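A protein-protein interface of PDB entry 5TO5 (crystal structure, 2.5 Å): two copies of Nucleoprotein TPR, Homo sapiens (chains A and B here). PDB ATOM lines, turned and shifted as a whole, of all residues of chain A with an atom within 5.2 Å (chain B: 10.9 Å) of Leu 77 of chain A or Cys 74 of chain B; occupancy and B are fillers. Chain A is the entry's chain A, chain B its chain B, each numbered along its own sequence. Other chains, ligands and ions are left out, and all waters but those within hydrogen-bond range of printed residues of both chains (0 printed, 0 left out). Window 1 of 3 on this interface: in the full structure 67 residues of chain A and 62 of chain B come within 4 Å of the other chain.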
ATOM      1  N   GLU A  70      -8.184  19.152  33.231  1.00  0.00           N
ATOM      2  CA  GLU A  70      -8.240  19.193  31.775  1.00  0.00           C
ATOM      3  C   GLU A  70      -9.331  20.141  31.293  1.00  0.00           C
ATOM      4  O   GLU A  70      -9.143  20.883  30.326  1.00  0.00           O
ATOM      5  CB  GLU A  70      -8.474  17.789  31.210  1.00  0.00           C
ATOM      6  CG  GLU A  70      -7.965  17.593  29.792  1.00  0.00           C
ATOM      7  CD  GLU A  70      -6.449  17.564  29.701  1.00  0.00           C
ATOM      8  OE1 GLU A  70      -5.783  17.457  30.752  1.00  0.00           O
ATOM      9  OE2 GLU A  70      -5.922  17.644  28.572  1.00  0.00           O
ATOM     10  N   GLU A  73      -8.070  23.595  31.721  1.00  0.00           N
ATOM     11  CA  GLU A  73      -7.087  23.927  30.696  1.00  0.00           C
ATOM     12  C   GLU A  73      -7.765  24.235  29.364  1.00  0.00           C
ATOM     13  O   GLU A  73      -7.358  25.149  28.644  1.00  0.00           O
ATOM     14  CB  GLU A  73      -6.090  22.781  30.531  1.00  0.00           C
ATOM     15  CG  GLU A  73      -5.045  22.998  29.448  1.00  0.00           C
ATOM     16  CD  GLU A  73      -3.853  23.798  29.921  1.00  0.00           C
ATOM     17  OE1 GLU A  73      -2.884  23.928  29.147  1.00  0.00           O
ATOM     18  OE2 GLU A  73      -3.883  24.294  31.064  1.00  0.00           O
ATOM     19  N   CYS A  74      -8.798  23.462  29.039  1.00  0.00           N
ATOM     20  CA  CYS A  74      -9.599  23.713  27.847  1.00  0.00           C
ATOM     21  C   CYS A  74     -10.162  25.124  27.844  1.00  0.00           C
ATOM     22  O   CYS A  74     -10.049  25.847  26.855  1.00  0.00           O
ATOM     23  CB  CYS A  74     -10.743  22.703  27.743  1.00  0.00           C
ATOM     24  SG  CYS A  74     -10.358  21.250  26.757  1.00  0.00           S
ATOM     25  N   GLN A  75     -10.762  25.511  28.963  1.00  0.00           N
ATOM     26  CA  GLN A  75     -11.383  26.823  29.076  1.00  0.00           C
ATOM     27  C   GLN A  75     -10.364  27.955  29.007  1.00  0.00           C
ATOM     28  O   GLN A  75     -10.669  29.030  28.495  1.00  0.00           O
ATOM     29  CB  GLN A  75     -12.185  26.919  30.372  1.00  0.00           C
ATOM     30  CG  GLN A  75     -13.510  26.188  30.305  1.00  0.00           C
ATOM     31  CD  GLN A  75     -14.008  25.753  31.662  1.00  0.00           C
ATOM     32  OE1 GLN A  75     -13.346  25.963  32.676  1.00  0.00           O
ATOM     33  NE2 GLN A  75     -15.182  25.133  31.687  1.00  0.00           N
ATOM     34  N   SER A  76      -9.157  27.715  29.511  1.00  0.00           N
ATOM     35  CA  SER A  76      -8.114  28.734  29.466  1.00  0.00           C
ATOM     36  C   SER A  76      -7.609  28.922  28.045  1.00  0.00           C
ATOM     37  O   SER A  76      -7.277  30.035  27.633  1.00  0.00           O
ATOM     38  CB  SER A  76      -6.957  28.373  30.396  1.00  0.00           C
ATOM     39  OG  SER A  76      -7.364  28.437  31.754  1.00  0.00           O
ATOM     40  N   LEU A  77      -7.555  27.823  27.302  1.00  0.00           N
ATOM     41  CA  LEU A  77      -7.144  27.857  25.904  1.00  0.00           C
ATOM     42  C   LEU A  77      -8.172  28.559  25.031  1.00  0.00           C
ATOM     43  O   LEU A  77      -7.821  29.318  24.134  1.00  0.00           O
ATOM     44  CB  LEU A  77      -6.907  26.441  25.388  1.00  0.00           C
ATOM     45  CG  LEU A  77      -5.555  25.861  25.796  1.00  0.00           C
ATOM     46  CD1 LEU A  77      -5.479  24.379  25.484  1.00  0.00           C
ATOM     47  CD2 LEU A  77      -4.443  26.613  25.090  1.00  0.00           C
ATOM     48  N   ARG A  78      -9.448  28.302  25.293  1.00  0.00           N
ATOM     49  CA  ARG A  78     -10.508  28.901  24.493  1.00  0.00           C
ATOM     50  C   ARG A  78     -10.499  30.416  24.621  1.00  0.00           C
ATOM     51  O   ARG A  78     -10.775  31.128  23.658  1.00  0.00           O
ATOM     52  CB  ARG A  78     -11.872  28.338  24.895  1.00  0.00           C
ATOM     53  CG  ARG A  78     -12.119  26.933  24.368  1.00  0.00           C
ATOM     54  CD  ARG A  78     -13.560  26.521  24.572  1.00  0.00           C
ATOM     55  NE  ARG A  78     -13.712  25.072  24.597  1.00  0.00           N
ATOM     56  CZ  ARG A  78     -13.741  24.346  25.710  1.00  0.00           C
ATOM     57  NH1 ARG A  78     -13.628  24.938  26.894  1.00  0.00           N
ATOM     58  NH2 ARG A  78     -13.881  23.030  25.646  1.00  0.00           N
ATOM     59  N   LEU A  79     -10.161  30.905  25.809  1.00  0.00           N
ATOM     60  CA  LEU A  79     -10.107  32.341  26.045  1.00  0.00           C
ATOM     61  C   LEU A  79      -8.972  33.003  25.268  1.00  0.00           C
ATOM     62  O   LEU A  79      -9.174  34.047  24.648  1.00  0.00           O
ATOM     63  CB  LEU A  79      -9.956  32.644  27.535  1.00  0.00           C
ATOM     64  CG  LEU A  79      -9.903  34.135  27.876  1.00  0.00           C
ATOM     65  CD1 LEU A  79     -11.175  34.834  27.418  1.00  0.00           C
ATOM     66  CD2 LEU A  79      -9.673  34.358  29.364  1.00  0.00           C
ATOM     67  N   GLU A  80      -7.779  32.411  25.296  1.00  0.00           N
ATOM     68  CA  GLU A  80      -6.646  33.024  24.610  1.00  0.00           C
ATOM     69  C   GLU A  80      -6.789  32.875  23.098  1.00  0.00           C
ATOM     70  O   GLU A  80      -6.258  33.687  22.339  1.00  0.00           O
ATOM     71  CB  GLU A  80      -5.308  32.441  25.095  1.00  0.00           C
ATOM     72  CG  GLU A  80      -5.296  30.950  25.393  1.00  0.00           C
ATOM     73  CD  GLU A  80      -3.992  30.496  26.037  1.00  0.00           C
ATOM     74  OE1 GLU A  80      -3.951  29.373  26.581  1.00  0.00           O
ATOM     75  OE2 GLU A  80      -3.004  31.262  25.999  1.00  0.00           O
ATOM     76  N   LEU A  81      -7.519  31.856  22.661  1.00  0.00           N
ATOM     77  CA  LEU A  81      -7.830  31.722  21.245  1.00  0.00           C
ATOM     78  C   LEU A  81      -8.753  32.853  20.795  1.00  0.00           C
ATOM     79  O   LEU A  81      -8.529  33.460  19.745  1.00  0.00           O
ATOM     80  CB  LEU A  81      -8.464  30.361  20.953  1.00  0.00           C
ATOM     81  CG  LEU A  81      -7.454  29.243  20.689  1.00  0.00           C
ATOM     82  CD1 LEU A  81      -8.026  27.889  21.054  1.00  0.00           C
ATOM     83  CD2 LEU A  81      -7.011  29.261  19.233  1.00  0.00           C
ATOM     84  N   GLU A  82      -9.775  33.143  21.597  1.00  0.00           N
ATOM     85  CA  GLU A  82     -10.729  34.199  21.272  1.00  0.00           C
ATOM     86  C   GLU A  82     -10.048  35.567  21.233  1.00  0.00           C
ATOM     87  O   GLU A  82     -10.328  36.381  20.354  1.00  0.00           O
ATOM     88  CB  GLU A  82     -11.888  34.206  22.276  1.00  0.00           C
ATOM     89  CG  GLU A  82     -13.050  35.124  21.892  1.00  0.00           C
ATOM     90  CD  GLU A  82     -14.306  34.871  22.711  1.00  0.00           C
ATOM     91  OE1 GLU A  82     -14.781  33.717  22.741  1.00  0.00           O
ATOM     92  OE2 GLU A  82     -14.824  35.828  23.325  1.00  0.00           O
ATOM     93  N   ARG B  66     -14.608  10.329  29.410  1.00  0.00           N
ATOM     94  CA  ARG B  66     -14.754  11.777  29.370  1.00  0.00           C
ATOM     95  C   ARG B  66     -13.410  12.479  29.543  1.00  0.00           C
ATOM     96  O   ARG B  66     -13.222  13.589  29.049  1.00  0.00           O
ATOM     97  CB  ARG B  66     -15.743  12.241  30.437  1.00  0.00           C
ATOM     98  CG  ARG B  66     -17.131  11.661  30.259  1.00  0.00           C
ATOM     99  CD  ARG B  66     -18.054  12.131  31.357  1.00  0.00           C
ATOM    100  NE  ARG B  66     -18.286  13.569  31.255  1.00  0.00           N
ATOM    101  CZ  ARG B  66     -18.456  14.371  32.300  1.00  0.00           C
ATOM    102  NH1 ARG B  66     -18.653  15.670  32.124  1.00  0.00           N
ATOM    103  NH2 ARG B  66     -18.420  13.867  33.524  1.00  0.00           N
ATOM    104  N   LEU B  67     -12.481  11.833  30.240  1.00  0.00           N
ATOM    105  CA  LEU B  67     -11.124  12.358  30.345  1.00  0.00           C
ATOM    106  C   LEU B  67     -10.410  12.256  28.999  1.00  0.00           C
ATOM    107  O   LEU B  67      -9.601  13.113  28.650  1.00  0.00           O
ATOM    108  CB  LEU B  67     -10.334  11.617  31.427  1.00  0.00           C
ATOM    109  CG  LEU B  67      -8.870  12.040  31.595  1.00  0.00           C
ATOM    110  CD1 LEU B  67      -8.765  13.528  31.900  1.00  0.00           C
ATOM    111  CD2 LEU B  67      -8.196  11.219  32.682  1.00  0.00           C
ATOM    112  N   VAL B  68     -10.715  11.202  28.247  1.00  0.00           N
ATOM    113  CA  VAL B  68     -10.146  11.024  26.918  1.00  0.00           C
ATOM    114  C   VAL B  68     -10.720  12.058  25.953  1.00  0.00           C
ATOM    115  O   VAL B  68      -9.992  12.649  25.157  1.00  0.00           O
ATOM    116  CB  VAL B  68     -10.403   9.604  26.375  1.00  0.00           C
ATOM    117  CG1 VAL B  68     -10.042   9.518  24.897  1.00  0.00           C
ATOM    118  CG2 VAL B  68      -9.612   8.584  27.175  1.00  0.00           C
ATOM    119  N   ASN B  69     -12.029  12.278  26.036  1.00  0.00           N
ATOM    120  CA  ASN B  69     -12.688  13.291  25.220  1.00  0.00           C
ATOM    121  C   ASN B  69     -12.118  14.682  25.471  1.00  0.00           C
ATOM    122  O   ASN B  69     -11.840  15.430  24.533  1.00  0.00           O
ATOM    123  CB  ASN B  69     -14.198  13.296  25.482  1.00  0.00           C
ATOM    124  CG  ASN B  69     -14.874  12.019  25.028  1.00  0.00           C
ATOM    125  OD1 ASN B  69     -14.249  11.161  24.409  1.00  0.00           O
ATOM    126  ND2 ASN B  69     -16.163  11.894  25.322  1.00  0.00           N
ATOM    127  N   GLU B  70     -11.931  15.014  26.744  1.00  0.00           N
ATOM    128  CA  GLU B  70     -11.501  16.349  27.134  1.00  0.00           C
ATOM    129  C   GLU B  70     -10.033  16.588  26.820  1.00  0.00           C
ATOM    130  O   GLU B  70      -9.627  17.709  26.524  1.00  0.00           O
ATOM    131  CB  GLU B  70     -11.756  16.572  28.625  1.00  0.00           C
ATOM    132  CG  GLU B  70     -11.858  18.035  29.031  1.00  0.00           C
ATOM    133  CD  GLU B  70     -13.188  18.672  28.656  1.00  0.00           C
ATOM    134  OE1 GLU B  70     -13.549  19.688  29.283  1.00  0.00           O
ATOM    135  OE2 GLU B  70     -13.878  18.171  27.743  1.00  0.00           O
ATOM    136  N   THR B  71      -9.237  15.529  26.894  1.00  0.00           N
ATOM    137  CA  THR B  71      -7.813  15.638  26.625  1.00  0.00           C
ATOM    138  C   THR B  71      -7.579  15.901  25.143  1.00  0.00           C
ATOM    139  O   THR B  71      -6.729  16.709  24.775  1.00  0.00           O
ATOM    140  CB  THR B  71      -7.063  14.370  27.062  1.00  0.00           C
ATOM    141  OG1 THR B  71      -7.417  14.052  28.413  1.00  0.00           O
ATOM    142  CG2 THR B  71      -5.557  14.577  26.968  1.00  0.00           C
ATOM    143  N   ARG B  72      -8.349  15.224  24.297  1.00  0.00           N
ATOM    144  CA  ARG B  72      -8.256  15.419  22.856  1.00  0.00           C
ATOM    145  C   ARG B  72      -8.639  16.837  22.454  1.00  0.00           C
ATOM    146  O   ARG B  72      -7.943  17.474  21.665  1.00  0.00           O
ATOM    147  CB  ARG B  72      -9.142  14.416  22.122  1.00  0.00           C
ATOM    148  CG  ARG B  72      -8.436  13.137  21.738  1.00  0.00           C
ATOM    149  CD  ARG B  72      -8.680  12.827  20.276  1.00  0.00           C
ATOM    150  NE  ARG B  72      -8.099  11.553  19.874  1.00  0.00           N
ATOM    151  CZ  ARG B  72      -8.255  11.020  18.669  1.00  0.00           C
ATOM    152  NH1 ARG B  72      -8.974  11.655  17.753  1.00  0.00           N
ATOM    153  NH2 ARG B  72      -7.695   9.855  18.378  1.00  0.00           N
ATOM    154  N   GLU B  73      -9.752  17.322  22.995  1.00  0.00           N
ATOM    155  CA  GLU B  73     -10.208  18.676  22.713  1.00  0.00           C
ATOM    156  C   GLU B  73      -9.167  19.695  23.159  1.00  0.00           C
ATOM    157  O   GLU B  73      -8.888  20.660  22.448  1.00  0.00           O
ATOM    158  CB  GLU B  73     -11.552  18.949  23.393  1.00  0.00           C
ATOM    159  CG  GLU B  73     -12.742  18.829  22.457  1.00  0.00           C
ATOM    160  CD  GLU B  73     -12.708  19.863  21.347  1.00  0.00           C
ATOM    161  OE1 GLU B  73     -12.381  21.032  21.639  1.00  0.00           O
ATOM    162  OE2 GLU B  73     -12.997  19.510  20.185  1.00  0.00           O
ATOM    163  N   CYS B  74      -8.589  19.460  24.331  1.00  0.00           N
ATOM    164  CA  CYS B  74      -7.554  20.328  24.874  1.00  0.00           C
ATOM    165  C   CYS B  74      -6.311  20.332  23.996  1.00  0.00           C
ATOM    166  O   CYS B  74      -5.707  21.378  23.760  1.00  0.00           O
ATOM    167  CB  CYS B  74      -7.192  19.887  26.289  1.00  0.00           C
ATOM    168  SG  CYS B  74      -5.777  20.750  26.985  1.00  0.00           S
ATOM    169  N   GLN B  75      -5.930  19.147  23.531  1.00  0.00           N
ATOM    170  CA  GLN B  75      -4.771  18.989  22.665  1.00  0.00           C
ATOM    171  C   GLN B  75      -4.998  19.706  21.339  1.00  0.00           C
ATOM    172  O   GLN B  75      -4.116  20.402  20.833  1.00  0.00           O
ATOM    173  CB  GLN B  75      -4.476  17.505  22.431  1.00  0.00           C
ATOM    174  CG  GLN B  75      -3.834  16.815  23.631  1.00  0.00           C
ATOM    175  CD  GLN B  75      -3.846  15.298  23.523  1.00  0.00           C
ATOM    176  OE1 GLN B  75      -4.620  14.723  22.759  1.00  0.00           O
ATOM    177  NE2 GLN B  75      -2.985  14.645  24.293  1.00  0.00           N
ATOM    178  N   SER B  76      -6.197  19.537  20.794  1.00  0.00           N
ATOM    179  CA  SER B  76      -6.595  20.197  19.557  1.00  0.00           C
ATOM    180  C   SER B  76      -6.695  21.711  19.736  1.00  0.00           C
ATOM    181  O   SER B  76      -6.536  22.469  18.783  1.00  0.00           O
ATOM    182  CB  SER B  76      -7.929  19.626  19.072  1.00  0.00           C
ATOM    183  OG  SER B  76      -8.490  20.418  18.044  1.00  0.00           O
ATOM    184  N   LEU B  77      -6.958  22.145  20.965  1.00  0.00           N
ATOM    185  CA  LEU B  77      -7.056  23.571  21.266  1.00  0.00           C
ATOM    186  C   LEU B  77      -5.683  24.228  21.272  1.00  0.00           C
ATOM    187  O   LEU B  77      -5.515  25.344  20.784  1.00  0.00           O
ATOM    188  CB  LEU B  77      -7.746  23.798  22.611  1.00  0.00           C
ATOM    189  CG  LEU B  77      -9.276  23.775  22.596  1.00  0.00           C
ATOM    190  CD1 LEU B  77      -9.812  23.867  24.013  1.00  0.00           C
ATOM    191  CD2 LEU B  77      -9.822  24.902  21.733  1.00  0.00           C
ATOM    192  N   ARG B  78      -4.706  23.532  21.843  1.00  0.00           N
ATOM    193  CA  ARG B  78      -3.321  23.975  21.770  1.00  0.00           C
ATOM    194  C   ARG B  78      -2.885  24.009  20.320  1.00  0.00           C
ATOM    195  O   ARG B  78      -2.180  24.918  19.886  1.00  0.00           O
ATOM    196  CB  ARG B  78      -2.406  23.053  22.573  1.00  0.00           C
ATOM    197  CG  ARG B  78      -2.109  23.561  23.950  1.00  0.00           C
ATOM    198  CD  ARG B  78      -0.685  24.079  24.086  1.00  0.00           C
ATOM    199  NE  ARG B  78      -0.556  25.094  25.131  1.00  0.00           N
ATOM    200  CZ  ARG B  78      -0.923  24.942  26.398  1.00  0.00           C
ATOM    201  NH1 ARG B  78      -1.448  23.810  26.821  1.00  0.00           N
ATOM    202  NH2 ARG B  78      -0.765  25.940  27.250  1.00  0.00           N
ATOM    203  N   LEU B  79      -3.309  22.991  19.587  1.00  0.00           N
ATOM    204  CA  LEU B  79      -3.039  22.875  18.168  1.00  0.00           C
ATOM    205  C   LEU B  79      -3.502  24.113  17.405  1.00  0.00           C
ATOM    206  O   LEU B  79      -2.755  24.697  16.621  1.00  0.00           O
ATOM    207  CB  LEU B  79      -3.736  21.626  17.623  1.00  0.00           C
ATOM    208  CG  LEU B  79      -3.707  21.458  16.119  1.00  0.00           C
ATOM    209  CD1 LEU B  79      -2.293  21.302  16.082  1.00  0.00           C
ATOM    210  CD2 LEU B  79      -4.307  20.170  15.624  1.00  0.00           C
ATOM    211  N   GLU B  80      -4.752  24.496  17.636  1.00  0.00           N
ATOM    212  CA  GLU B  80      -5.317  25.689  17.024  1.00  0.00           C
ATOM    213  C   GLU B  80      -4.559  26.941  17.449  1.00  0.00           C
ATOM    214  O   GLU B  80      -4.390  27.872  16.661  1.00  0.00           O
ATOM    215  CB  GLU B  80      -6.798  25.831  17.390  1.00  0.00           C
ATOM    216  CG  GLU B  80      -7.694  24.752  16.814  1.00  0.00           C
ATOM    217  CD  GLU B  80      -9.136  24.894  17.255  1.00  0.00           C
ATOM    218  OE1 GLU B  80      -9.403  25.701  18.166  1.00  0.00           O
ATOM    219  OE2 GLU B  80     -10.002  24.198  16.690  1.00  0.00           O
ATOM    220  N   LEU B  81      -4.105  26.957  18.698  1.00  0.00           N
ATOM    221  CA  LEU B  81      -3.471  28.139  19.265  1.00  0.00           C
ATOM    222  C   LEU B  81      -2.035  28.300  18.785  1.00  0.00           C
ATOM    223  O   LEU B  81      -1.501  29.411  18.744  1.00  0.00           O
ATOM    224  CB  LEU B  81      -3.507  28.077  20.792  1.00  0.00           C
ATOM    225  CG  LEU B  81      -2.829  29.228  21.538  1.00  0.00           C
ATOM    226  CD1 LEU B  81      -3.522  30.542  21.231  1.00  0.00           C
ATOM    227  CD2 LEU B  81      -2.808  28.972  23.027  1.00  0.00           C
ATOM    228  N   GLU B  82      -1.409  27.189  18.418  1.00  0.00           N
ATOM    229  CA  GLU B  82      -0.041  27.219  17.921  1.00  0.00           C
ATOM    230  C   GLU B  82      -0.002  27.782  16.507  1.00  0.00           C
ATOM    231  O   GLU B  82       0.806  28.657  16.194  1.00  0.00           O
ATOM    232  CB  GLU B  82       0.569  25.816  17.956  1.00  0.00           C
ATOM    233  CG  GLU B  82       2.043  25.762  17.593  1.00  0.00           C
ATOM    234  CD  GLU B  82       2.952  26.081  18.766  1.00  0.00           C
ATOM    235  OE1 GLU B  82       2.732  27.107  19.441  1.00  0.00           O
ATOM    236  OE2 GLU B  82       3.889  25.295  19.016  1.00  0.00           O
ATOM    237  N   LYS B  83      -0.887  27.266  15.663  1.00  0.00           N
ATOM    238  CA  LYS B  83      -1.018  27.726  14.286  1.00  0.00           C
ATOM    239  C   LYS B  83      -1.384  29.205  14.247  1.00  0.00           C
ATOM    240  O   LYS B  83      -0.930  29.949  13.379  1.00  0.00           O
ATOM    241  CB  LYS B  83      -2.070  26.887  13.553  1.00  0.00           C
ATOM    242  CG  LYS B  83      -2.257  27.229  12.081  1.00  0.00           C
ATOM    243  CD  LYS B  83      -3.526  28.035  11.848  1.00  0.00           C
ATOM    244  CE  LYS B  83      -3.840  28.146  10.364  1.00  0.00           C
ATOM    245  NZ  LYS B  83      -4.042  26.806   9.747  1.00  0.00           N
ATOM    246  N   LEU B  84      -2.199  29.623  15.207  1.00  0.00           N
ATOM    247  CA  LEU B  84      -2.651  31.005  15.299  1.00  0.00           C
ATOM    248  C   LEU B  84      -1.533  31.945  15.753  1.00  0.00           C
ATOM    249  O   LEU B  84      -1.434  33.071  15.277  1.00  0.00           O
ATOM    250  CB  LEU B  84      -3.849  31.095  16.251  1.00  0.00           C
ATOM    251  CG  LEU B  84      -4.507  32.452  16.485  1.00  0.00           C
ATOM    252  CD1 LEU B  84      -4.773  33.153  15.169  1.00  0.00           C
ATOM    253  CD2 LEU B  84      -5.805  32.260  17.248  1.00  0.00           C
ATOM    254  N   ASN B  85      -0.693  31.481  16.672  1.00  0.00           N
ATOM    255  CA  ASN B  85       0.451  32.272  17.120  1.00  0.00           C
ATOM    256  C   ASN B  85       1.480  32.484  16.015  1.00  0.00           C
ATOM    257  O   ASN B  85       2.116  33.535  15.946  1.00  0.00           O
ATOM    258  CB  ASN B  85       1.121  31.614  18.326  1.00  0.00           C
ATOM    259  CG  ASN B  85       0.642  32.188  19.644  1.00  0.00           C
ATOM    260  OD1 ASN B  85       0.332  33.379  19.743  1.00  0.00           O
ATOM    261  ND2 ASN B  85       0.584  31.345  20.669  1.00  0.00           N
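SG of Cys 74 of chain A lies close to O of Glu 70 of chain A (3.8 Å). The side-chain amide nitrogen (ND2) of Asn 85 of chain B sits at hydrogen-bond distance from the backbone carbonyl oxygen (O) of Leu 81 of chain B (3.4 Å).
Glu 70 of chain A touches Glu 70 of chain B. Cys 74 of chain B touches Glu 73 of chain A. Leu 77 of chain B touches Cys 74 of chain A. CD1 of Leu 77 of chain A touches O of Cys 74 of chain B, at 3.5 Å. Leu 77 of chain A touches Arg 78 of chain B (CD1 to CG, 3.8 Å). Leu 77 of chain A touches Leu 81 of chain B. Leu 81 of chain B touches Glu 80 of chain A (CD2 to CD, 3.6 Å). Leu 77 of chain B touches Leu 81 of chain A (CD2 to CD1, 3.6 Å). Leu 81 of chain A touches Glu 80 of chain B. CD2 of Leu 81 of chain A touches CA of Leu 81 of chain B, at 3.7 Å.
O of Glu 70 of chain B is in hydrogen-bond range of SG of Cys 74 of chain A. OE1 of Glu 73 of chain A lies within salt-bridge range of NH1 of Arg 78 of chain B, at 2.7 Å. OE2 of Glu 70 of chain A sits close to SG of Cys 74 of chain B, 3.5 Å away. The side-chain sulfur (SG) of Cys 74 of chain A lies close to the backbone NH (N) of Cys 74 of chain B (3.5 Å).
Of chain B, only Cys 74 (3.5 Å), Leu 77 (3.7 Å), Arg 78 (3.8 Å) and Leu 81 (3.5 Å) come within 4 Å of Leu 77 of chain A. Of chain A, only Glu 70 (3.4 Å), Glu 73 (3.4 Å), Cys 74 (3.5 Å) and Leu 77 (3.5 Å) come within 4 Å of Cys 74 of chain B. Of chain B, only Cys 74 and Arg 78 come within 4 Å of Glu 73 of chain A. Of chain B, only Glu 70 (3.6 Å), Cys 74 (3.5 Å) and Leu 77 (3.5 Å) come within 4 Å of Cys 74 of chain A. Glu 80 of chain A touches just one residue of chain B: Leu 81. Leu 81 of chain A touches just these residues of chain B: Leu 77, Glu 80, Leu 81 and Leu 84. Of the printed residues of chain B, Glu 70 of chain A touches Glu 70 (3.7 Å), Thr 71 (3.4 Å) and Cys 74 (3.4 Å). Of the printed residues of chain A, Arg 78 of chain B touches Glu 73 (2.7 Å) and Leu 77 (3.8 Å). Asn 85 of chain B touches none of the printed residues of chain A. Leu 79 of chain B touches none of the printed residues of chain A. The nearest printed residue of chain A that does not touch Cys 74 of chain B is Arg 78 of chain A (6.5 Å). The nearest printed residue of chain A that does not touch Leu 77 of chain B is Gln 75 of chain A (5.3 Å).
Hydrophobic or aromatic side chains of chain A within 4 Å of the printed part of chain B: Leu 77 and Leu 81. Of the 20 printed residues of chain B, 8 touch a printed residue of chain A. Among the printed residues, Asp or Glu carboxylates within 4 Å of a Lys or Arg side-chain nitrogen of the other chain: Glu 73 of chain A with Arg 78 of chain B.
Glu 73 of chain A touches Cys 74 of chain B, but with the chains exchanged Cys 74 of chain A does not touch Glu 73 of chain B (4.1 Å). Cys 74 of chain B touches its own counterpart, Cys 74 of chain A. Leu 77 of chain A touches its own counterpart, Leu 77 of chain B. Leu 81 of chain B touches its own counterpart, Leu 81 of chain A. Positions printed for both chains: 70, 73, 74, 75, 76, 77, 78, 79, 80, 81 and 82.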
